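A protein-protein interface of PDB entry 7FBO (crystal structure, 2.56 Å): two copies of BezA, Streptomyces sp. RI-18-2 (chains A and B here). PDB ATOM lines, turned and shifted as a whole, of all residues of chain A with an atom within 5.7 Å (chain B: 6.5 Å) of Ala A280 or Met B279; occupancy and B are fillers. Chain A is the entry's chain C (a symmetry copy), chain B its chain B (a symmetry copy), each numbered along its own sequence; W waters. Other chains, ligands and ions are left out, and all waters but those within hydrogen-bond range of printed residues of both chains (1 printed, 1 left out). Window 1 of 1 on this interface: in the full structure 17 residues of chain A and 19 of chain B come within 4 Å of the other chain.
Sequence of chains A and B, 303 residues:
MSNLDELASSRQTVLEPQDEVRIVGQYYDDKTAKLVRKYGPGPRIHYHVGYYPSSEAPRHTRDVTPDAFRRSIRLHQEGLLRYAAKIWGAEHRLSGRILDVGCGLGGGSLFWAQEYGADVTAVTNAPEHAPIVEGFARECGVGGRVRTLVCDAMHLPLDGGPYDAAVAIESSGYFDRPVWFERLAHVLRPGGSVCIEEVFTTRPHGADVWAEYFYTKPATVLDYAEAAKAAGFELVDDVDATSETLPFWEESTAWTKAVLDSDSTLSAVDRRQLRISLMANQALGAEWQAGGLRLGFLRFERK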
ATOM      1  N   VAL A 209      24.132  -4.235  11.440  1.00  0.00           N
ATOM      2  CA  VAL A 209      24.452  -3.399  10.289  1.00  0.00           C
ATOM      3  C   VAL A 209      25.550  -4.062   9.464  1.00  0.00           C
ATOM      4  O   VAL A 209      25.445  -4.198   8.241  1.00  0.00           O
ATOM      5  CB  VAL A 209      24.846  -1.984  10.752  1.00  0.00           C
ATOM      6  CG1 VAL A 209      25.460  -1.208   9.616  1.00  0.00           C
ATOM      7  CG2 VAL A 209      23.637  -1.253  11.303  1.00  0.00           C
ATOM      8  N   TRP A 210      26.598  -4.528  10.137  1.00  0.00           N
ATOM      9  CA  TRP A 210      27.667  -5.255   9.466  1.00  0.00           C
ATOM     10  C   TRP A 210      27.139  -6.515   8.797  1.00  0.00           C
ATOM     11  O   TRP A 210      27.519  -6.834   7.663  1.00  0.00           O
ATOM     12  CB  TRP A 210      28.753  -5.597  10.488  1.00  0.00           C
ATOM     13  CG  TRP A 210      29.762  -6.597  10.033  1.00  0.00           C
ATOM     14  CD1 TRP A 210      29.612  -7.939  10.012  1.00  0.00           C
ATOM     15  CD2 TRP A 210      31.096  -6.336   9.565  1.00  0.00           C
ATOM     16  NE1 TRP A 210      30.751  -8.540   9.557  1.00  0.00           N
ATOM     17  CE2 TRP A 210      31.682  -7.581   9.277  1.00  0.00           C
ATOM     18  CE3 TRP A 210      31.845  -5.171   9.359  1.00  0.00           C
ATOM     19  CZ2 TRP A 210      32.985  -7.707   8.792  1.00  0.00           C
ATOM     20  CZ3 TRP A 210      33.141  -5.289   8.883  1.00  0.00           C
ATOM     21  CH2 TRP A 210      33.700  -6.552   8.605  1.00  0.00           C
ATOM     22  N   TYR A 213      24.537  -5.930   5.720  1.00  0.00           N
ATOM     23  CA  TYR A 213      25.124  -5.232   4.587  1.00  0.00           C
ATOM     24  C   TYR A 213      26.165  -6.085   3.883  1.00  0.00           C
ATOM     25  O   TYR A 213      26.358  -5.945   2.664  1.00  0.00           O
ATOM     26  CB  TYR A 213      25.754  -3.915   5.054  1.00  0.00           C
ATOM     27  CG  TYR A 213      26.355  -3.075   3.953  1.00  0.00           C
ATOM     28  CD1 TYR A 213      25.558  -2.481   2.984  1.00  0.00           C
ATOM     29  CD2 TYR A 213      27.725  -2.844   3.900  1.00  0.00           C
ATOM     30  CE1 TYR A 213      26.114  -1.689   1.983  1.00  0.00           C
ATOM     31  CE2 TYR A 213      28.287  -2.066   2.903  1.00  0.00           C
ATOM     32  CZ  TYR A 213      27.477  -1.498   1.947  1.00  0.00           C
ATOM     33  OH  TYR A 213      28.048  -0.730   0.951  1.00  0.00           O
ATOM     34  N   TRP A 249      36.864   3.417   9.731  1.00  0.00           N
ATOM     35  CA  TRP A 249      35.605   3.885   9.173  1.00  0.00           C
ATOM     36  C   TRP A 249      35.667   5.361   8.853  1.00  0.00           C
ATOM     37  O   TRP A 249      35.064   5.809   7.868  1.00  0.00           O
ATOM     38  CB  TRP A 249      34.454   3.584  10.142  1.00  0.00           C
ATOM     39  CG  TRP A 249      34.330   2.121  10.336  1.00  0.00           C
ATOM     40  CD1 TRP A 249      34.665   1.407  11.448  1.00  0.00           C
ATOM     41  CD2 TRP A 249      33.922   1.171   9.352  1.00  0.00           C
ATOM     42  NE1 TRP A 249      34.458   0.065  11.220  1.00  0.00           N
ATOM     43  CE2 TRP A 249      33.996  -0.102   9.944  1.00  0.00           C
ATOM     44  CE3 TRP A 249      33.475   1.276   8.034  1.00  0.00           C
ATOM     45  CZ2 TRP A 249      33.654  -1.248   9.269  1.00  0.00           C
ATOM     46  CZ3 TRP A 249      33.130   0.140   7.371  1.00  0.00           C
ATOM     47  CH2 TRP A 249      33.222  -1.108   7.984  1.00  0.00           C
ATOM     48  N   ARG A 275      27.568   7.101  -3.007  1.00  0.00           N
ATOM     49  CA  ARG A 275      26.680   7.628  -1.978  1.00  0.00           C
ATOM     50  C   ARG A 275      26.184   6.519  -1.060  1.00  0.00           C
ATOM     51  O   ARG A 275      26.255   6.642   0.167  1.00  0.00           O
ATOM     52  CB  ARG A 275      25.498   8.350  -2.614  1.00  0.00           C
ATOM     53  CG  ARG A 275      24.445   8.736  -1.596  1.00  0.00           C
ATOM     54  CD  ARG A 275      25.066   9.527  -0.462  1.00  0.00           C
ATOM     55  NE  ARG A 275      25.786  10.676  -0.981  1.00  0.00           N
ATOM     56  CZ  ARG A 275      26.299  11.643  -0.237  1.00  0.00           C
ATOM     57  NH1 ARG A 275      26.215  11.616   1.088  1.00  0.00           N
ATOM     58  NH2 ARG A 275      26.896  12.667  -0.839  1.00  0.00           N
ATOM     59  N   ILE A 276      25.661   5.433  -1.635  1.00  0.00           N
ATOM     60  CA  ILE A 276      25.197   4.321  -0.808  1.00  0.00           C
ATOM     61  C   ILE A 276      26.342   3.780   0.038  1.00  0.00           C
ATOM     62  O   ILE A 276      26.158   3.482   1.220  1.00  0.00           O
ATOM     63  CB  ILE A 276      24.557   3.221  -1.676  1.00  0.00           C
ATOM     64  CG1 ILE A 276      23.252   3.713  -2.308  1.00  0.00           C
ATOM     65  CG2 ILE A 276      24.313   1.954  -0.856  1.00  0.00           C
ATOM     66  CD1 ILE A 276      22.506   2.616  -3.072  1.00  0.00           C
ATOM     67  N   SER A 277      27.553   3.703  -0.532  1.00  0.00           N
ATOM     68  CA  SER A 277      28.702   3.264   0.255  1.00  0.00           C
ATOM     69  C   SER A 277      28.972   4.205   1.423  1.00  0.00           C
ATOM     70  O   SER A 277      29.266   3.753   2.535  1.00  0.00           O
ATOM     71  CB  SER A 277      29.946   3.146  -0.618  1.00  0.00           C
ATOM     72  OG  SER A 277      30.996   2.555   0.141  1.00  0.00           O
ATOM     73  N   LEU A 278      28.887   5.515   1.185  1.00  0.00           N
ATOM     74  CA  LEU A 278      29.096   6.486   2.250  1.00  0.00           C
ATOM     75  C   LEU A 278      28.031   6.331   3.323  1.00  0.00           C
ATOM     76  O   LEU A 278      28.330   6.349   4.526  1.00  0.00           O
ATOM     77  CB  LEU A 278      29.083   7.908   1.682  1.00  0.00           C
ATOM     78  CG  LEU A 278      29.940   9.006   2.336  1.00  0.00           C
ATOM     79  CD1 LEU A 278      29.834  10.266   1.523  1.00  0.00           C
ATOM     80  CD2 LEU A 278      29.511   9.309   3.745  1.00  0.00           C
ATOM     81  N   MET A 279      26.778   6.167   2.903  1.00  0.00           N
ATOM     82  CA  MET A 279      25.705   6.028   3.875  1.00  0.00           C
ATOM     83  C   MET A 279      25.941   4.805   4.734  1.00  0.00           C
ATOM     84  O   MET A 279      25.735   4.840   5.954  1.00  0.00           O
ATOM     85  CB  MET A 279      24.361   5.945   3.162  1.00  0.00           C
ATOM     86  CG  MET A 279      24.050   7.212   2.387  1.00  0.00           C
ATOM     87  SD  MET A 279      22.485   7.154   1.500  1.00  0.00           S
ATOM     88  CE  MET A 279      22.429   5.448   1.023  1.00  0.00           C
ATOM     89  N   ALA A 280      26.425   3.728   4.119  1.00  0.00           N
ATOM     90  CA  ALA A 280      26.716   2.510   4.860  1.00  0.00           C
ATOM     91  C   ALA A 280      27.923   2.690   5.774  1.00  0.00           C
ATOM     92  O   ALA A 280      27.939   2.176   6.901  1.00  0.00           O
ATOM     93  CB  ALA A 280      26.956   1.361   3.895  1.00  0.00           C
ATOM     94  N   ASN A 281      28.953   3.398   5.309  1.00  0.00           N
ATOM     95  CA  ASN A 281      30.136   3.533   6.145  1.00  0.00           C
ATOM     96  C   ASN A 281      29.826   4.301   7.414  1.00  0.00           C
ATOM     97  O   ASN A 281      30.434   4.046   8.463  1.00  0.00           O
ATOM     98  CB  ASN A 281      31.254   4.199   5.365  1.00  0.00           C
ATOM     99  CG  ASN A 281      32.110   3.185   4.651  1.00  0.00           C
ATOM    100  OD1 ASN A 281      33.123   2.722   5.184  1.00  0.00           O
ATOM    101  ND2 ASN A 281      31.680   2.791   3.453  1.00  0.00           N
ATOM    102  N   GLN A 282      28.876   5.231   7.344  1.00  0.00           N
ATOM    103  CA  GLN A 282      28.510   5.981   8.533  1.00  0.00           C
ATOM    104  C   GLN A 282      27.750   5.099   9.520  1.00  0.00           C
ATOM    105  O   GLN A 282      28.018   5.133  10.726  1.00  0.00           O
ATOM    106  CB  GLN A 282      27.689   7.198   8.128  1.00  0.00           C
ATOM    107  CG  GLN A 282      28.465   8.183   7.281  1.00  0.00           C
ATOM    108  CD  GLN A 282      27.613   9.356   6.823  1.00  0.00           C
ATOM    109  OE1 GLN A 282      26.403   9.211   6.578  1.00  0.00           O
ATOM    110  NE2 GLN A 282      28.236  10.528   6.710  1.00  0.00           N
ATOM    111  N   ALA A 283      26.814   4.288   9.021  1.00  0.00           N
ATOM    112  CA  ALA A 283      26.061   3.412   9.902  1.00  0.00           C
ATOM    113  C   ALA A 283      26.933   2.287  10.453  1.00  0.00           C
ATOM    114  O   ALA A 283      26.708   1.823  11.581  1.00  0.00           O
ATOM    115  CB  ALA A 283      24.848   2.854   9.155  1.00  0.00           C
ATOM    116  N   LEU A 284      27.927   1.836   9.677  1.00  0.00           N
ATOM    117  CA  LEU A 284      28.868   0.839  10.170  1.00  0.00           C
ATOM    118  C   LEU A 284      29.772   1.435  11.234  1.00  0.00           C
ATOM    119  O   LEU A 284      30.056   0.792  12.255  1.00  0.00           O
ATOM    120  CB  LEU A 284      29.709   0.299   9.024  1.00  0.00           C
ATOM    121  CG  LEU A 284      28.957  -0.640   8.088  1.00  0.00           C
ATOM    122  CD1 LEU A 284      29.695  -0.765   6.733  1.00  0.00           C
ATOM    123  CD2 LEU A 284      28.756  -1.991   8.743  1.00  0.00           C
ATOM    124  N   GLY A 285      30.240   2.662  11.004  1.00  0.00           N
ATOM    125  CA  GLY A 285      31.057   3.327  11.995  1.00  0.00           C
ATOM    126  C   GLY A 285      30.295   3.615  13.270  1.00  0.00           C
ATOM    127  O   GLY A 285      30.876   3.573  14.360  1.00  0.00           O
ATOM    128  N   ARG B 272      19.838  -8.389   2.581  1.00  0.00           N
ATOM    129  CA  ARG B 272      20.903  -7.419   2.345  1.00  0.00           C
ATOM    130  C   ARG B 272      20.374  -6.161   1.660  1.00  0.00           C
ATOM    131  O   ARG B 272      20.815  -5.047   1.975  1.00  0.00           O
ATOM    132  CB  ARG B 272      22.004  -8.067   1.520  1.00  0.00           C
ATOM    133  CG  ARG B 272      22.944  -7.109   0.837  1.00  0.00           C
ATOM    134  CD  ARG B 272      24.327  -7.716   0.709  1.00  0.00           C
ATOM    135  NE  ARG B 272      25.297  -6.754   0.213  1.00  0.00           N
ATOM    136  CZ  ARG B 272      25.286  -6.241  -1.014  1.00  0.00           C
ATOM    137  NH1 ARG B 272      24.387  -6.614  -1.907  1.00  0.00           N
ATOM    138  NH2 ARG B 272      26.197  -5.328  -1.347  1.00  0.00           N
ATOM    139  N   LEU B 274      17.294  -4.991   2.086  1.00  0.00           N
ATOM    140  CA  LEU B 274      16.655  -4.272   3.181  1.00  0.00           C
ATOM    141  C   LEU B 274      17.686  -3.572   4.049  1.00  0.00           C
ATOM    142  O   LEU B 274      17.462  -2.442   4.492  1.00  0.00           O
ATOM    143  CB  LEU B 274      15.812  -5.215   4.033  1.00  0.00           C
ATOM    144  CG  LEU B 274      14.420  -5.474   3.460  1.00  0.00           C
ATOM    145  CD1 LEU B 274      13.847  -6.802   3.992  1.00  0.00           C
ATOM    146  CD2 LEU B 274      13.499  -4.303   3.751  1.00  0.00           C
ATOM    147  N   ARG B 275      18.817  -4.229   4.313  1.00  0.00           N
ATOM    148  CA  ARG B 275      19.831  -3.618   5.165  1.00  0.00           C
ATOM    149  C   ARG B 275      20.354  -2.332   4.533  1.00  0.00           C
ATOM    150  O   ARG B 275      20.488  -1.297   5.208  1.00  0.00           O
ATOM    151  CB  ARG B 275      20.972  -4.602   5.416  1.00  0.00           C
ATOM    152  CG  ARG B 275      22.207  -3.990   6.062  1.00  0.00           C
ATOM    153  CD  ARG B 275      21.846  -3.171   7.319  1.00  0.00           C
ATOM    154  NE  ARG B 275      21.275  -3.978   8.392  1.00  0.00           N
ATOM    155  CZ  ARG B 275      20.879  -3.505   9.566  1.00  0.00           C
ATOM    156  NH1 ARG B 275      21.003  -2.223   9.868  1.00  0.00           N
ATOM    157  NH2 ARG B 275      20.334  -4.340  10.456  1.00  0.00           N
ATOM    158  N   ILE B 276      20.638  -2.385   3.225  1.00  0.00           N
ATOM    159  CA  ILE B 276      21.167  -1.228   2.510  1.00  0.00           C
ATOM    160  C   ILE B 276      20.167  -0.083   2.550  1.00  0.00           C
ATOM    161  O   ILE B 276      20.544   1.082   2.708  1.00  0.00           O
ATOM    162  CB  ILE B 276      21.543  -1.614   1.065  1.00  0.00           C
ATOM    163  CG1 ILE B 276      22.860  -2.401   1.050  1.00  0.00           C
ATOM    164  CG2 ILE B 276      21.579  -0.377   0.150  1.00  0.00           C
ATOM    165  CD1 ILE B 276      23.134  -3.134  -0.229  1.00  0.00           C
ATOM    166  N   SER B 277      18.877  -0.402   2.436  1.00  0.00           N
ATOM    167  CA  SER B 277      17.841   0.618   2.538  1.00  0.00           C
ATOM    168  C   SER B 277      17.831   1.259   3.919  1.00  0.00           C
ATOM    169  O   SER B 277      17.549   2.461   4.054  1.00  0.00           O
ATOM    170  CB  SER B 277      16.481   0.005   2.217  1.00  0.00           C
ATOM    171  OG  SER B 277      15.466   0.976   2.327  1.00  0.00           O
ATOM    172  N   LEU B 278      18.134   0.473   4.961  1.00  0.00           N
ATOM    173  CA  LEU B 278      18.193   1.038   6.308  1.00  0.00           C
ATOM    174  C   LEU B 278      19.361   2.007   6.431  1.00  0.00           C
ATOM    175  O   LEU B 278      19.184   3.140   6.898  1.00  0.00           O
ATOM    176  CB  LEU B 278      18.286  -0.068   7.361  1.00  0.00           C
ATOM    177  CG  LEU B 278      17.562   0.184   8.699  1.00  0.00           C
ATOM    178  CD1 LEU B 278      17.379  -1.125   9.475  1.00  0.00           C
ATOM    179  CD2 LEU B 278      18.272   1.214   9.566  1.00  0.00           C
ATOM    180  N   MET B 279      20.563   1.596   5.985  1.00  0.00           N
ATOM    181  CA  MET B 279      21.697   2.524   5.996  1.00  0.00           C
ATOM    182  C   MET B 279      21.387   3.775   5.184  1.00  0.00           C
ATOM    183  O   MET B 279      21.772   4.884   5.569  1.00  0.00           O
ATOM    184  CB  MET B 279      22.958   1.856   5.464  1.00  0.00           C
ATOM    185  CG  MET B 279      23.155   0.438   5.921  1.00  0.00           C
ATOM    186  SD  MET B 279      24.252  -0.498   4.841  1.00  0.00           S
ATOM    187  CE  MET B 279      25.263  -1.305   6.056  1.00  0.00           C
ATOM    188  N   ALA B 280      20.669   3.613   4.068  1.00  0.00           N
ATOM    189  CA  ALA B 280      20.286   4.752   3.242  1.00  0.00           C
ATOM    190  C   ALA B 280      19.343   5.682   3.987  1.00  0.00           C
ATOM    191  O   ALA B 280      19.548   6.902   4.025  1.00  0.00           O
ATOM    192  CB  ALA B 280      19.620   4.263   1.958  1.00  0.00           C
ATOM    193  N   ASN B 281      18.282   5.114   4.563  1.00  0.00           N
ATOM    194  CA  ASN B 281      17.332   5.909   5.329  1.00  0.00           C
ATOM    195  C   ASN B 281      18.032   6.636   6.458  1.00  0.00           C
ATOM    196  O   ASN B 281      17.727   7.799   6.736  1.00  0.00           O
ATOM    197  CB  ASN B 281      16.225   5.005   5.855  1.00  0.00           C
ATOM    198  CG  ASN B 281      15.157   4.774   4.827  1.00  0.00           C
ATOM    199  OD1 ASN B 281      14.115   5.424   4.837  1.00  0.00           O
ATOM    200  ND2 ASN B 281      15.437   3.885   3.887  1.00  0.00           N
ATOM    201  N   GLN B 282      19.010   5.987   7.090  1.00  0.00           N
ATOM    202  CA  GLN B 282      19.754   6.669   8.143  1.00  0.00           C
ATOM    203  C   GLN B 282      20.579   7.824   7.584  1.00  0.00           C
ATOM    204  O   GLN B 282      20.662   8.889   8.209  1.00  0.00           O
ATOM    205  CB  GLN B 282      20.652   5.684   8.882  1.00  0.00           C
ATOM    206  CG  GLN B 282      19.947   4.961  10.008  1.00  0.00           C
ATOM    207  CD  GLN B 282      20.678   3.697  10.424  1.00  0.00           C
ATOM    208  OE1 GLN B 282      21.750   3.379   9.887  1.00  0.00           O
ATOM    209  NE2 GLN B 282      20.124   2.988  11.412  1.00  0.00           N
ATOM    210  N   ALA B 283      21.202   7.641   6.413  1.00  0.00           N
ATOM    211  CA  ALA B 283      21.960   8.743   5.827  1.00  0.00           C
ATOM    212  C   ALA B 283      21.035   9.804   5.256  1.00  0.00           C
ATOM    213  O   ALA B 283      21.350  11.001   5.314  1.00  0.00           O
ATOM    214  CB  ALA B 283      22.903   8.224   4.750  1.00  0.00           C
ATOM    215  N   LEU B 284      19.874   9.388   4.741  1.00  0.00           N
ATOM    216  CA  LEU B 284      18.940  10.344   4.153  1.00  0.00           C
ATOM    217  C   LEU B 284      18.333  11.244   5.225  1.00  0.00           C
ATOM    218  O   LEU B 284      18.297  12.470   5.065  1.00  0.00           O
ATOM    219  CB  LEU B 284      17.856   9.600   3.379  1.00  0.00           C
ATOM    220  CG  LEU B 284      18.363   9.027   2.053  1.00  0.00           C
ATOM    221  CD1 LEU B 284      17.470   7.899   1.533  1.00  0.00           C
ATOM    222  CD2 LEU B 284      18.513  10.142   1.017  1.00  0.00           C
HETATM  223  O   HOH W   1      23.719   6.232   7.262  1.00  0.00           O
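Water W1 lies within hydrogen-bond range of O of Met A279, O of Met B279 and N of Ala B283.
Among the printed residues, merely in contact across the chains: Val A209 with Arg B275, Val A209 with Met B279, Tyr A213 with Arg B275, Tyr A213 with Ile B276, Tyr A213 with Met B279, Ile A276 with Ile B276, Met A279 with Met B279, Met A279 with Ala B280, Met A279 with Ala B283, Ala A280 with Met B279 and Ala A283 with Gln B282.
O of Tyr A213 lies within hydrogen-bond range of NE of Arg B272, at 2.8 Å.
Ile B276 touches its own counterpart, Ile A276.
Met A279 touches Ala B280, and with the chains exchanged Ala A280 touches Met B279.
Met A279 touches Ala B283, but with the chains exchanged Ala A283 does not touch Met B279 (4.3 Å).
Ala A283 touches Gln B282, but with the chains exchanged Gln A282 does not touch Ala B283 (4.1 Å).
Of the 12 pairs that touch across the chains among the printed residues, 4 have their exchanged pair printed and touching as well.
Of the 12 printed residues of chain B, 7 touch a printed residue of chain A.
Hydrophobic or aromatic side chains of chain B that line the printed part of chain A: Ile B276, Met B279, Ala B280 and Ala B283.
Printed residues of chain A that touch a printed residue of chain B: Val A209, Tyr A213, Ile A276, Met A279, Ala A280 and Ala A283.
Hydrophobic or aromatic side chains of chain A that line the printed part of chain B: Val A209, Tyr A213, Ile A276, Met A279, Ala A280 and Ala A283.
Among the printed residues, 12 pairs touch across the chains.
Ala A280 touches just one residue of chain B: Met B279 (3.4 Å).
Met B279 touches four residues of chain A.
Printed residues of chain A within 4 Å of Ala B280: Met A279 (3.2 Å).
Printed residues of chain B within 4 Å of Met A279: Met B279, Ala B280 and Ala B283.
The nearest printed residue of chain B that does not touch Ala A280 is Ala B283 (5.7 Å).
The nearest printed residue of chain A that does not touch Met B279 is Ala A283 (4.3 Å).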
